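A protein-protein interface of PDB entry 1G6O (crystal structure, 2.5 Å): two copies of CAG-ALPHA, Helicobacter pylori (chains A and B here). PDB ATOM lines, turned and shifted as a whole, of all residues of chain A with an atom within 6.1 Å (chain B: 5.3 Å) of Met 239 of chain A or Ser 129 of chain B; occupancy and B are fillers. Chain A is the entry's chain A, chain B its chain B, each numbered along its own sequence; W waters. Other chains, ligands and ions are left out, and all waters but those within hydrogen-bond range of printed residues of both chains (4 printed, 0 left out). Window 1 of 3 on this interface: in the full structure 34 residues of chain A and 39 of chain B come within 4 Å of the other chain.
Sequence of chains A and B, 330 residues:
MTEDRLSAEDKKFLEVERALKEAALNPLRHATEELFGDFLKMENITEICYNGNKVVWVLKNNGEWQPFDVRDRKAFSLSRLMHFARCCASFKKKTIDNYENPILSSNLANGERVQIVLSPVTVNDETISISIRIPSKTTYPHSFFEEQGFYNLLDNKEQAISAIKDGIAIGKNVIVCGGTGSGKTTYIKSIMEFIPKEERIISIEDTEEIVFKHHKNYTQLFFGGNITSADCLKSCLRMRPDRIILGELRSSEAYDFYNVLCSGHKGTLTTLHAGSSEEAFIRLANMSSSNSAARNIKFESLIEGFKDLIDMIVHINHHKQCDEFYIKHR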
ATOM      1  N   ARG A 200      20.275  18.162  28.873  1.00  0.00           N
ATOM      2  CA  ARG A 200      21.227  17.652  27.892  1.00  0.00           C
ATOM      3  C   ARG A 200      22.091  16.756  28.748  1.00  0.00           C
ATOM      4  O   ARG A 200      22.617  17.210  29.771  1.00  0.00           O
ATOM      5  CB  ARG A 200      22.088  18.770  27.282  1.00  0.00           C
ATOM      6  CG  ARG A 200      23.197  18.269  26.341  1.00  0.00           C
ATOM      7  CD  ARG A 200      23.797  19.392  25.484  1.00  0.00           C
ATOM      8  NE  ARG A 200      25.080  19.049  24.862  1.00  0.00           N
ATOM      9  CZ  ARG A 200      25.222  18.266  23.792  1.00  0.00           C
ATOM     10  NH1 ARG A 200      24.162  17.728  23.200  1.00  0.00           N
ATOM     11  NH2 ARG A 200      26.434  18.018  23.302  1.00  0.00           N
ATOM     12  N   ILE A 202      25.351  13.924  29.046  1.00  0.00           N
ATOM     13  CA  ILE A 202      26.589  13.427  28.465  1.00  0.00           C
ATOM     14  C   ILE A 202      27.196  12.337  29.369  1.00  0.00           C
ATOM     15  O   ILE A 202      27.527  12.604  30.521  1.00  0.00           O
ATOM     16  CB  ILE A 202      27.629  14.572  28.239  1.00  0.00           C
ATOM     17  CG1 ILE A 202      27.044  15.602  27.278  1.00  0.00           C
ATOM     18  CG2 ILE A 202      28.954  14.007  27.635  1.00  0.00           C
ATOM     19  CD1 ILE A 202      27.975  16.724  26.995  1.00  0.00           C
ATOM     20  N   THR A 219      24.776  12.751  24.255  1.00  0.00           N
ATOM     21  CA  THR A 219      25.940  12.283  23.501  1.00  0.00           C
ATOM     22  C   THR A 219      26.669  11.322  24.427  1.00  0.00           C
ATOM     23  O   THR A 219      26.873  11.633  25.608  1.00  0.00           O
ATOM     24  CB  THR A 219      26.979  13.415  23.130  1.00  0.00           C
ATOM     25  OG1 THR A 219      26.380  14.347  22.236  1.00  0.00           O
ATOM     26  CG2 THR A 219      28.234  12.814  22.435  1.00  0.00           C
ATOM     27  N   LEU A 221      30.100   9.190  25.351  1.00  0.00           N
ATOM     28  CA  LEU A 221      31.553   9.298  25.202  1.00  0.00           C
ATOM     29  C   LEU A 221      32.146   8.010  25.741  1.00  0.00           C
ATOM     30  O   LEU A 221      31.726   7.551  26.806  1.00  0.00           O
ATOM     31  CB  LEU A 221      32.108  10.484  25.998  1.00  0.00           C
ATOM     32  CG  LEU A 221      31.849  11.901  25.474  1.00  0.00           C
ATOM     33  CD1 LEU A 221      32.540  12.912  26.410  1.00  0.00           C
ATOM     34  CD2 LEU A 221      32.329  12.006  23.997  1.00  0.00           C
ATOM     35  N   CYS A 232      37.994  12.204  28.039  1.00  0.00           N
ATOM     36  CA  CYS A 232      36.550  12.321  27.815  1.00  0.00           C
ATOM     37  C   CYS A 232      35.888  13.360  28.717  1.00  0.00           C
ATOM     38  O   CYS A 232      35.095  14.182  28.252  1.00  0.00           O
ATOM     39  CB  CYS A 232      35.882  10.980  28.065  1.00  0.00           C
ATOM     40  SG  CYS A 232      36.562   9.686  27.062  1.00  0.00           S
ATOM     41  N   SER A 235      36.776  16.712  27.591  1.00  0.00           N
ATOM     42  CA  SER A 235      36.085  17.026  26.350  1.00  0.00           C
ATOM     43  C   SER A 235      34.638  17.329  26.710  1.00  0.00           C
ATOM     44  O   SER A 235      34.025  18.233  26.178  1.00  0.00           O
ATOM     45  CB  SER A 235      36.142  15.830  25.399  1.00  0.00           C
ATOM     46  OG  SER A 235      35.537  16.119  24.146  1.00  0.00           O
ATOM     47  N   CYS A 236      34.103  16.550  27.629  1.00  0.00           N
ATOM     48  CA  CYS A 236      32.741  16.712  28.072  1.00  0.00           C
ATOM     49  C   CYS A 236      32.430  18.135  28.573  1.00  0.00           C
ATOM     50  O   CYS A 236      31.333  18.673  28.382  1.00  0.00           O
ATOM     51  CB  CYS A 236      32.499  15.696  29.168  1.00  0.00           C
ATOM     52  SG  CYS A 236      30.967  15.908  30.040  1.00  0.00           S
ATOM     53  N   LEU A 237      33.403  18.758  29.209  1.00  0.00           N
ATOM     54  CA  LEU A 237      33.189  20.085  29.732  1.00  0.00           C
ATOM     55  C   LEU A 237      33.149  21.181  28.678  1.00  0.00           C
ATOM     56  O   LEU A 237      32.820  22.334  28.973  1.00  0.00           O
ATOM     57  CB  LEU A 237      34.249  20.369  30.787  1.00  0.00           C
ATOM     58  CG  LEU A 237      33.975  19.514  32.029  1.00  0.00           C
ATOM     59  CD1 LEU A 237      35.039  19.820  33.066  1.00  0.00           C
ATOM     60  CD2 LEU A 237      32.559  19.791  32.589  1.00  0.00           C
ATOM     61  N   ARG A 238      33.476  20.797  27.444  1.00  0.00           N
ATOM     62  CA  ARG A 238      33.496  21.692  26.282  1.00  0.00           C
ATOM     63  C   ARG A 238      32.279  21.399  25.379  1.00  0.00           C
ATOM     64  O   ARG A 238      32.150  21.969  24.303  1.00  0.00           O
ATOM     65  CB  ARG A 238      34.819  21.508  25.491  1.00  0.00           C
ATOM     66  CG  ARG A 238      36.117  21.910  26.244  1.00  0.00           C
ATOM     67  CD  ARG A 238      36.055  23.344  26.876  1.00  0.00           C
ATOM     68  NE  ARG A 238      35.767  24.430  25.922  1.00  0.00           N
ATOM     69  CZ  ARG A 238      34.595  25.071  25.804  1.00  0.00           C
ATOM     70  NH1 ARG A 238      33.557  24.761  26.583  1.00  0.00           N
ATOM     71  NH2 ARG A 238      34.449  26.029  24.888  1.00  0.00           N
ATOM     72  N   MET A 239      31.373  20.546  25.858  1.00  0.00           N
ATOM     73  CA  MET A 239      30.188  20.158  25.110  1.00  0.00           C
ATOM     74  C   MET A 239      28.853  20.540  25.779  1.00  0.00           C
ATOM     75  O   MET A 239      27.824  19.884  25.559  1.00  0.00           O
ATOM     76  CB  MET A 239      30.230  18.663  24.871  1.00  0.00           C
ATOM     77  CG  MET A 239      31.476  18.217  24.126  1.00  0.00           C
ATOM     78  SD  MET A 239      31.794  16.302  24.382  1.00  0.00           S
ATOM     79  CE  MET A 239      30.479  15.652  23.110  1.00  0.00           C
ATOM     80  N   ARG A 240      28.904  21.588  26.612  1.00  0.00           N
ATOM     81  CA  ARG A 240      27.756  22.165  27.352  1.00  0.00           C
ATOM     82  C   ARG A 240      26.686  21.187  27.909  1.00  0.00           C
ATOM     83  O   ARG A 240      25.519  21.266  27.534  1.00  0.00           O
ATOM     84  CB  ARG A 240      27.065  23.204  26.451  1.00  0.00           C
ATOM     85  CG  ARG A 240      26.000  24.050  27.133  1.00  0.00           C
ATOM     86  CD  ARG A 240      26.637  25.140  27.957  1.00  0.00           C
ATOM     87  NE  ARG A 240      26.904  26.298  27.131  1.00  0.00           N
ATOM     88  CZ  ARG A 240      26.308  27.477  27.281  1.00  0.00           C
ATOM     89  NH1 ARG A 240      25.415  27.663  28.243  1.00  0.00           N
ATOM     90  NH2 ARG A 240      26.576  28.464  26.435  1.00  0.00           N
ATOM     91  N   PRO A 241      27.057  20.293  28.851  1.00  0.00           N
ATOM     92  CA  PRO A 241      26.076  19.348  29.390  1.00  0.00           C
ATOM     93  C   PRO A 241      25.198  19.900  30.510  1.00  0.00           C
ATOM     94  O   PRO A 241      25.559  20.849  31.180  1.00  0.00           O
ATOM     95  CB  PRO A 241      26.963  18.220  29.888  1.00  0.00           C
ATOM     96  CG  PRO A 241      28.073  18.982  30.523  1.00  0.00           C
ATOM     97  CD  PRO A 241      28.383  20.040  29.452  1.00  0.00           C
ATOM     98  N   GLU B  47      24.729  28.281  22.318  1.00  0.00           N
ATOM     99  CA  GLU B  47      25.458  27.081  21.930  1.00  0.00           C
ATOM    100  C   GLU B  47      24.757  26.395  20.765  1.00  0.00           C
ATOM    101  O   GLU B  47      23.543  26.544  20.587  1.00  0.00           O
ATOM    102  CB  GLU B  47      25.550  26.118  23.127  1.00  0.00           C
ATOM    103  CG  GLU B  47      26.517  24.926  23.000  1.00  0.00           C
ATOM    104  CD  GLU B  47      27.947  25.221  23.496  1.00  0.00           C
ATOM    105  OE1 GLU B  47      28.107  26.111  24.380  1.00  0.00           O
ATOM    106  OE2 GLU B  47      28.901  24.544  23.026  1.00  0.00           O
ATOM    107  N   CYS B  49      24.732  22.521  18.976  1.00  0.00           N
ATOM    108  CA  CYS B  49      25.233  21.153  19.073  1.00  0.00           C
ATOM    109  C   CYS B  49      24.614  20.227  18.068  1.00  0.00           C
ATOM    110  O   CYS B  49      23.414  20.262  17.879  1.00  0.00           O
ATOM    111  CB  CYS B  49      24.924  20.546  20.440  1.00  0.00           C
ATOM    112  SG  CYS B  49      25.900  21.166  21.802  1.00  0.00           S
ATOM    113  N   TYR B  50      25.440  19.392  17.445  1.00  0.00           N
ATOM    114  CA  TYR B  50      24.970  18.368  16.532  1.00  0.00           C
ATOM    115  C   TYR B  50      25.428  17.103  17.270  1.00  0.00           C
ATOM    116  O   TYR B  50      26.608  16.984  17.631  1.00  0.00           O
ATOM    117  CB  TYR B  50      25.629  18.473  15.148  1.00  0.00           C
ATOM    118  CG  TYR B  50      25.184  17.377  14.203  1.00  0.00           C
ATOM    119  CD1 TYR B  50      23.871  17.329  13.740  1.00  0.00           C
ATOM    120  CD2 TYR B  50      26.054  16.339  13.833  1.00  0.00           C
ATOM    121  CE1 TYR B  50      23.418  16.282  12.940  1.00  0.00           C
ATOM    122  CE2 TYR B  50      25.610  15.273  13.019  1.00  0.00           C
ATOM    123  CZ  TYR B  50      24.283  15.263  12.579  1.00  0.00           C
ATOM    124  OH  TYR B  50      23.812  14.277  11.746  1.00  0.00           O
ATOM    125  N   ASN B  51      24.496  16.181  17.522  1.00  0.00           N
ATOM    126  CA  ASN B  51      24.788  14.947  18.267  1.00  0.00           C
ATOM    127  C   ASN B  51      24.992  13.720  17.381  1.00  0.00           C
ATOM    128  O   ASN B  51      24.869  12.579  17.843  1.00  0.00           O
ATOM    129  CB  ASN B  51      23.655  14.660  19.261  1.00  0.00           C
ATOM    130  CG  ASN B  51      23.554  15.703  20.370  1.00  0.00           C
ATOM    131  OD1 ASN B  51      22.579  15.723  21.113  1.00  0.00           O
ATOM    132  ND2 ASN B  51      24.556  16.562  20.485  1.00  0.00           N
ATOM    133  N   GLY B  52      25.278  13.961  16.106  1.00  0.00           N
ATOM    134  CA  GLY B  52      25.516  12.881  15.165  1.00  0.00           C
ATOM    135  C   GLY B  52      24.298  12.072  14.795  1.00  0.00           C
ATOM    136  O   GLY B  52      24.425  10.965  14.268  1.00  0.00           O
ATOM    137  N   GLN B 115      34.194  21.999  19.430  1.00  0.00           N
ATOM    138  CA  GLN B 115      34.660  20.726  19.945  1.00  0.00           C
ATOM    139  C   GLN B 115      34.089  19.622  19.046  1.00  0.00           C
ATOM    140  O   GLN B 115      32.881  19.542  18.838  1.00  0.00           O
ATOM    141  CB  GLN B 115      34.178  20.557  21.384  1.00  0.00           C
ATOM    142  CG  GLN B 115      34.768  19.400  22.161  1.00  0.00           C
ATOM    143  CD  GLN B 115      36.237  19.589  22.511  1.00  0.00           C
ATOM    144  OE1 GLN B 115      36.806  20.667  22.332  1.00  0.00           O
ATOM    145  NE2 GLN B 115      36.854  18.539  23.015  1.00  0.00           N
ATOM    146  N   ILE B 116      34.967  18.785  18.497  1.00  0.00           N
ATOM    147  CA  ILE B 116      34.568  17.684  17.614  1.00  0.00           C
ATOM    148  C   ILE B 116      35.075  16.334  18.090  1.00  0.00           C
ATOM    149  O   ILE B 116      36.252  16.182  18.412  1.00  0.00           O
ATOM    150  CB  ILE B 116      35.105  17.895  16.202  1.00  0.00           C
ATOM    151  CG1 ILE B 116      34.726  19.295  15.726  1.00  0.00           C
ATOM    152  CG2 ILE B 116      34.546  16.823  15.261  1.00  0.00           C
ATOM    153  CD1 ILE B 116      35.137  19.606  14.310  1.00  0.00           C
ATOM    154  N   VAL B 117      34.178  15.351  18.133  1.00  0.00           N
ATOM    155  CA  VAL B 117      34.536  13.992  18.551  1.00  0.00           C
ATOM    156  C   VAL B 117      34.154  12.944  17.484  1.00  0.00           C
ATOM    157  O   VAL B 117      33.064  12.980  16.922  1.00  0.00           O
ATOM    158  CB  VAL B 117      33.872  13.631  19.901  1.00  0.00           C
ATOM    159  CG1 VAL B 117      34.521  12.367  20.449  1.00  0.00           C
ATOM    160  CG2 VAL B 117      34.030  14.789  20.891  1.00  0.00           C
ATOM    161  N   THR B 122      33.017   8.377  19.952  1.00  0.00           N
ATOM    162  CA  THR B 122      31.570   8.498  19.842  1.00  0.00           C
ATOM    163  C   THR B 122      31.043   7.053  19.908  1.00  0.00           C
ATOM    164  O   THR B 122      31.825   6.100  19.943  1.00  0.00           O
ATOM    165  CB  THR B 122      31.141   9.221  18.522  1.00  0.00           C
ATOM    166  OG1 THR B 122      31.657   8.544  17.374  1.00  0.00           O
ATOM    167  CG2 THR B 122      31.638  10.648  18.531  1.00  0.00           C
ATOM    168  N   THR B 127      28.483   8.249  13.734  1.00  0.00           N
ATOM    169  CA  THR B 127      28.263   9.329  14.684  1.00  0.00           C
ATOM    170  C   THR B 127      29.400  10.371  14.845  1.00  0.00           C
ATOM    171  O   THR B 127      30.471  10.082  15.384  1.00  0.00           O
ATOM    172  CB  THR B 127      27.885   8.760  16.117  1.00  0.00           C
ATOM    173  OG1 THR B 127      26.727   7.931  16.036  1.00  0.00           O
ATOM    174  CG2 THR B 127      27.530   9.874  17.067  1.00  0.00           C
ATOM    175  N   ILE B 128      29.163  11.584  14.353  1.00  0.00           N
ATOM    176  CA  ILE B 128      30.133  12.661  14.531  1.00  0.00           C
ATOM    177  C   ILE B 128      29.476  13.739  15.435  1.00  0.00           C
ATOM    178  O   ILE B 128      28.384  14.245  15.159  1.00  0.00           O
ATOM    179  CB  ILE B 128      30.578  13.252  13.173  1.00  0.00           C
ATOM    180  CG1 ILE B 128      31.335  12.168  12.399  1.00  0.00           C
ATOM    181  CG2 ILE B 128      31.417  14.513  13.369  1.00  0.00           C
ATOM    182  CD1 ILE B 128      31.755  12.617  11.027  1.00  0.00           C
ATOM    183  N   SER B 129      30.134  14.047  16.543  1.00  0.00           N
ATOM    184  CA  SER B 129      29.631  15.022  17.493  1.00  0.00           C
ATOM    185  C   SER B 129      30.356  16.374  17.399  1.00  0.00           C
ATOM    186  O   SER B 129      31.591  16.435  17.459  1.00  0.00           O
ATOM    187  CB  SER B 129      29.777  14.456  18.900  1.00  0.00           C
ATOM    188  OG  SER B 129      29.537  15.459  19.866  1.00  0.00           O
ATOM    189  N   ILE B 130      29.582  17.451  17.273  1.00  0.00           N
ATOM    190  CA  ILE B 130      30.134  18.803  17.159  1.00  0.00           C
ATOM    191  C   ILE B 130      29.374  19.720  18.096  1.00  0.00           C
ATOM    192  O   ILE B 130      28.162  19.579  18.252  1.00  0.00           O
ATOM    193  CB  ILE B 130      29.968  19.383  15.714  1.00  0.00           C
ATOM    194  CG1 ILE B 130      30.501  18.385  14.690  1.00  0.00           C
ATOM    195  CG2 ILE B 130      30.669  20.744  15.617  1.00  0.00           C
ATOM    196  CD1 ILE B 130      30.250  18.787  13.265  1.00  0.00           C
ATOM    197  N   SER B 131      30.078  20.652  18.726  1.00  0.00           N
ATOM    198  CA  SER B 131      29.425  21.618  19.596  1.00  0.00           C
ATOM    199  C   SER B 131      30.166  22.949  19.514  1.00  0.00           C
ATOM    200  O   SER B 131      31.376  23.013  19.700  1.00  0.00           O
ATOM    201  CB  SER B 131      29.323  21.084  21.037  1.00  0.00           C
ATOM    202  OG  SER B 131      30.533  20.509  21.460  1.00  0.00           O
HETATM  203  O   HOH W   1      31.256  24.374  23.790  1.00  0.00           O
HETATM  204  O   HOH W   2      26.970  16.752  20.601  1.00  0.00           O
HETATM  205  O   HOH W   3      35.983  23.592  22.720  1.00  0.00           O
HETATM  206  O   HOH W   4      33.149  24.444  22.156  1.00  0.00           O
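Printed residues of chain A that touch a printed residue of chain B: Arg 200, Thr 219, Ser 235, Arg 238, Met 239 and Arg 240. Hydrophobic or aromatic side chains of chain A within 4 Å of the printed part of chain B: Met 239. Along chain A the printed residues that touch a printed residue of chain B span positions 200 to 240. Of the 14 printed residues of chain B, 7 touch a printed residue of chain A. Among the printed residues, Asp or Glu carboxylates within 4 Å of a Lys or Arg side-chain nitrogen of the other chain: Arg 240 of chain A with Glu 47 of chain B (3.0 Å).
Among the printed residues, pairs that only touch across the chains: Met 239 of chain A with Ser 129 of chain B, Arg 238 of chain A with Ser 131 of chain B, Met 239 of chain A with Ser 131 of chain B, Arg 238 of chain A with Gln 115 of chain B, Ser 235 of chain A with Val 117 of chain B and Thr 219 of chain A with Ser 129 of chain B.
Water W2 lies within hydrogen-bond range of the side-chain amide nitrogen of Asn 51 of chain B (2.4 Å), the side-chain hydroxyl of Thr 219 of chain A (3.0 Å), the side-chain hydroxyl of Ser 129 of chain B (3.0 Å), the backbone carbonyl oxygen of Tyr 50 of chain B (3.0 Å) and the guanidinium group of Arg 200 of chain A (3.0 Å). Water W1 lies within hydrogen-bond range of the side-chain carboxylate (OE2) of Glu 47 of chain B (2.5 Å) and the backbone carbonyl oxygen (O) of Arg 238 of chain A (2.6 Å). Water W3 lies within hydrogen-bond range of the side-chain amide oxygen of Gln 115 of chain B (3.1 Å) and the guanidinium group of Arg 238 of chain A (3.3 Å). Water W4 lies within hydrogen-bond range of O of Ser 131 of chain B (3.4 Å) and NH2 of Arg 238 of chain A (3.4 Å).
The side-chain carboxylate of Glu 47 of chain B lies within salt-bridge range of the guanidinium group of Arg 240 of chain A, at 3.0 Å. The side-chain amide nitrogen (ND2) of Asn 51 of chain B sits close to the guanidinium group (NH1) of Arg 200 of chain A (3.0 Å). NH2 of Arg 200 of chain A lies within hydrogen-bond range of SG of Cys 49 of chain B (3.5 Å). The side-chain hydroxyl (OG1) of Thr 219 of chain A is in hydrogen-bond range of the side-chain amide nitrogen (ND2) of Asn 51 of chain B (3.4 Å). The side-chain hydroxyl of Ser 235 of chain A lies within hydrogen-bond range of the side-chain amide nitrogen of Gln 115 of chain B (3.0 Å).
The backbone carbonyl oxygen (O) of Ser 131 of chain B lies within hydrogen-bond range of the backbone NH (N) of Gln 115 of chain B, at 3.0 Å. The side-chain hydroxyl (OG) of Ser 235 of chain A lies within hydrogen-bond range of the side-chain sulfur (SD) of Met 239 of chain A, 3.8 Å away. O of Arg 240 of chain A sits close to NE of Arg 200 of chain A. O of Met 239 of chain A lies within hydrogen-bond range of NE of Arg 200 of chain A. The backbone carbonyl oxygen (O) of Ser 129 of chain B is in hydrogen-bond range of the backbone NH (N) of Val 117 of chain B (2.9 Å).
Of the printed residues of chain B, Met 239 of chain A touches Ser 129 (3.4 Å) and Ser 131 (3.6 Å). Of the printed residues of chain A, Ser 129 of chain B touches Thr 219 and Met 239. Printed residues of chain A within 4 Å of Asn 51 of chain B: Arg 200 and Thr 219. Of the printed residues of chain B, Ser 235 of chain A touches Gln 115 (3.0 Å) and Val 117 (3.8 Å). Thr 127 of chain B touches none of the printed residues of chain A. The nearest residue of chain A that does not touch Ser 129 of chain B is Arg 200 of chain A (5.3 Å).
No position is printed for both chains. Of the 11 pairs that touch across the chains among the printed residues, none has its exchanged pair printed and touching as well.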
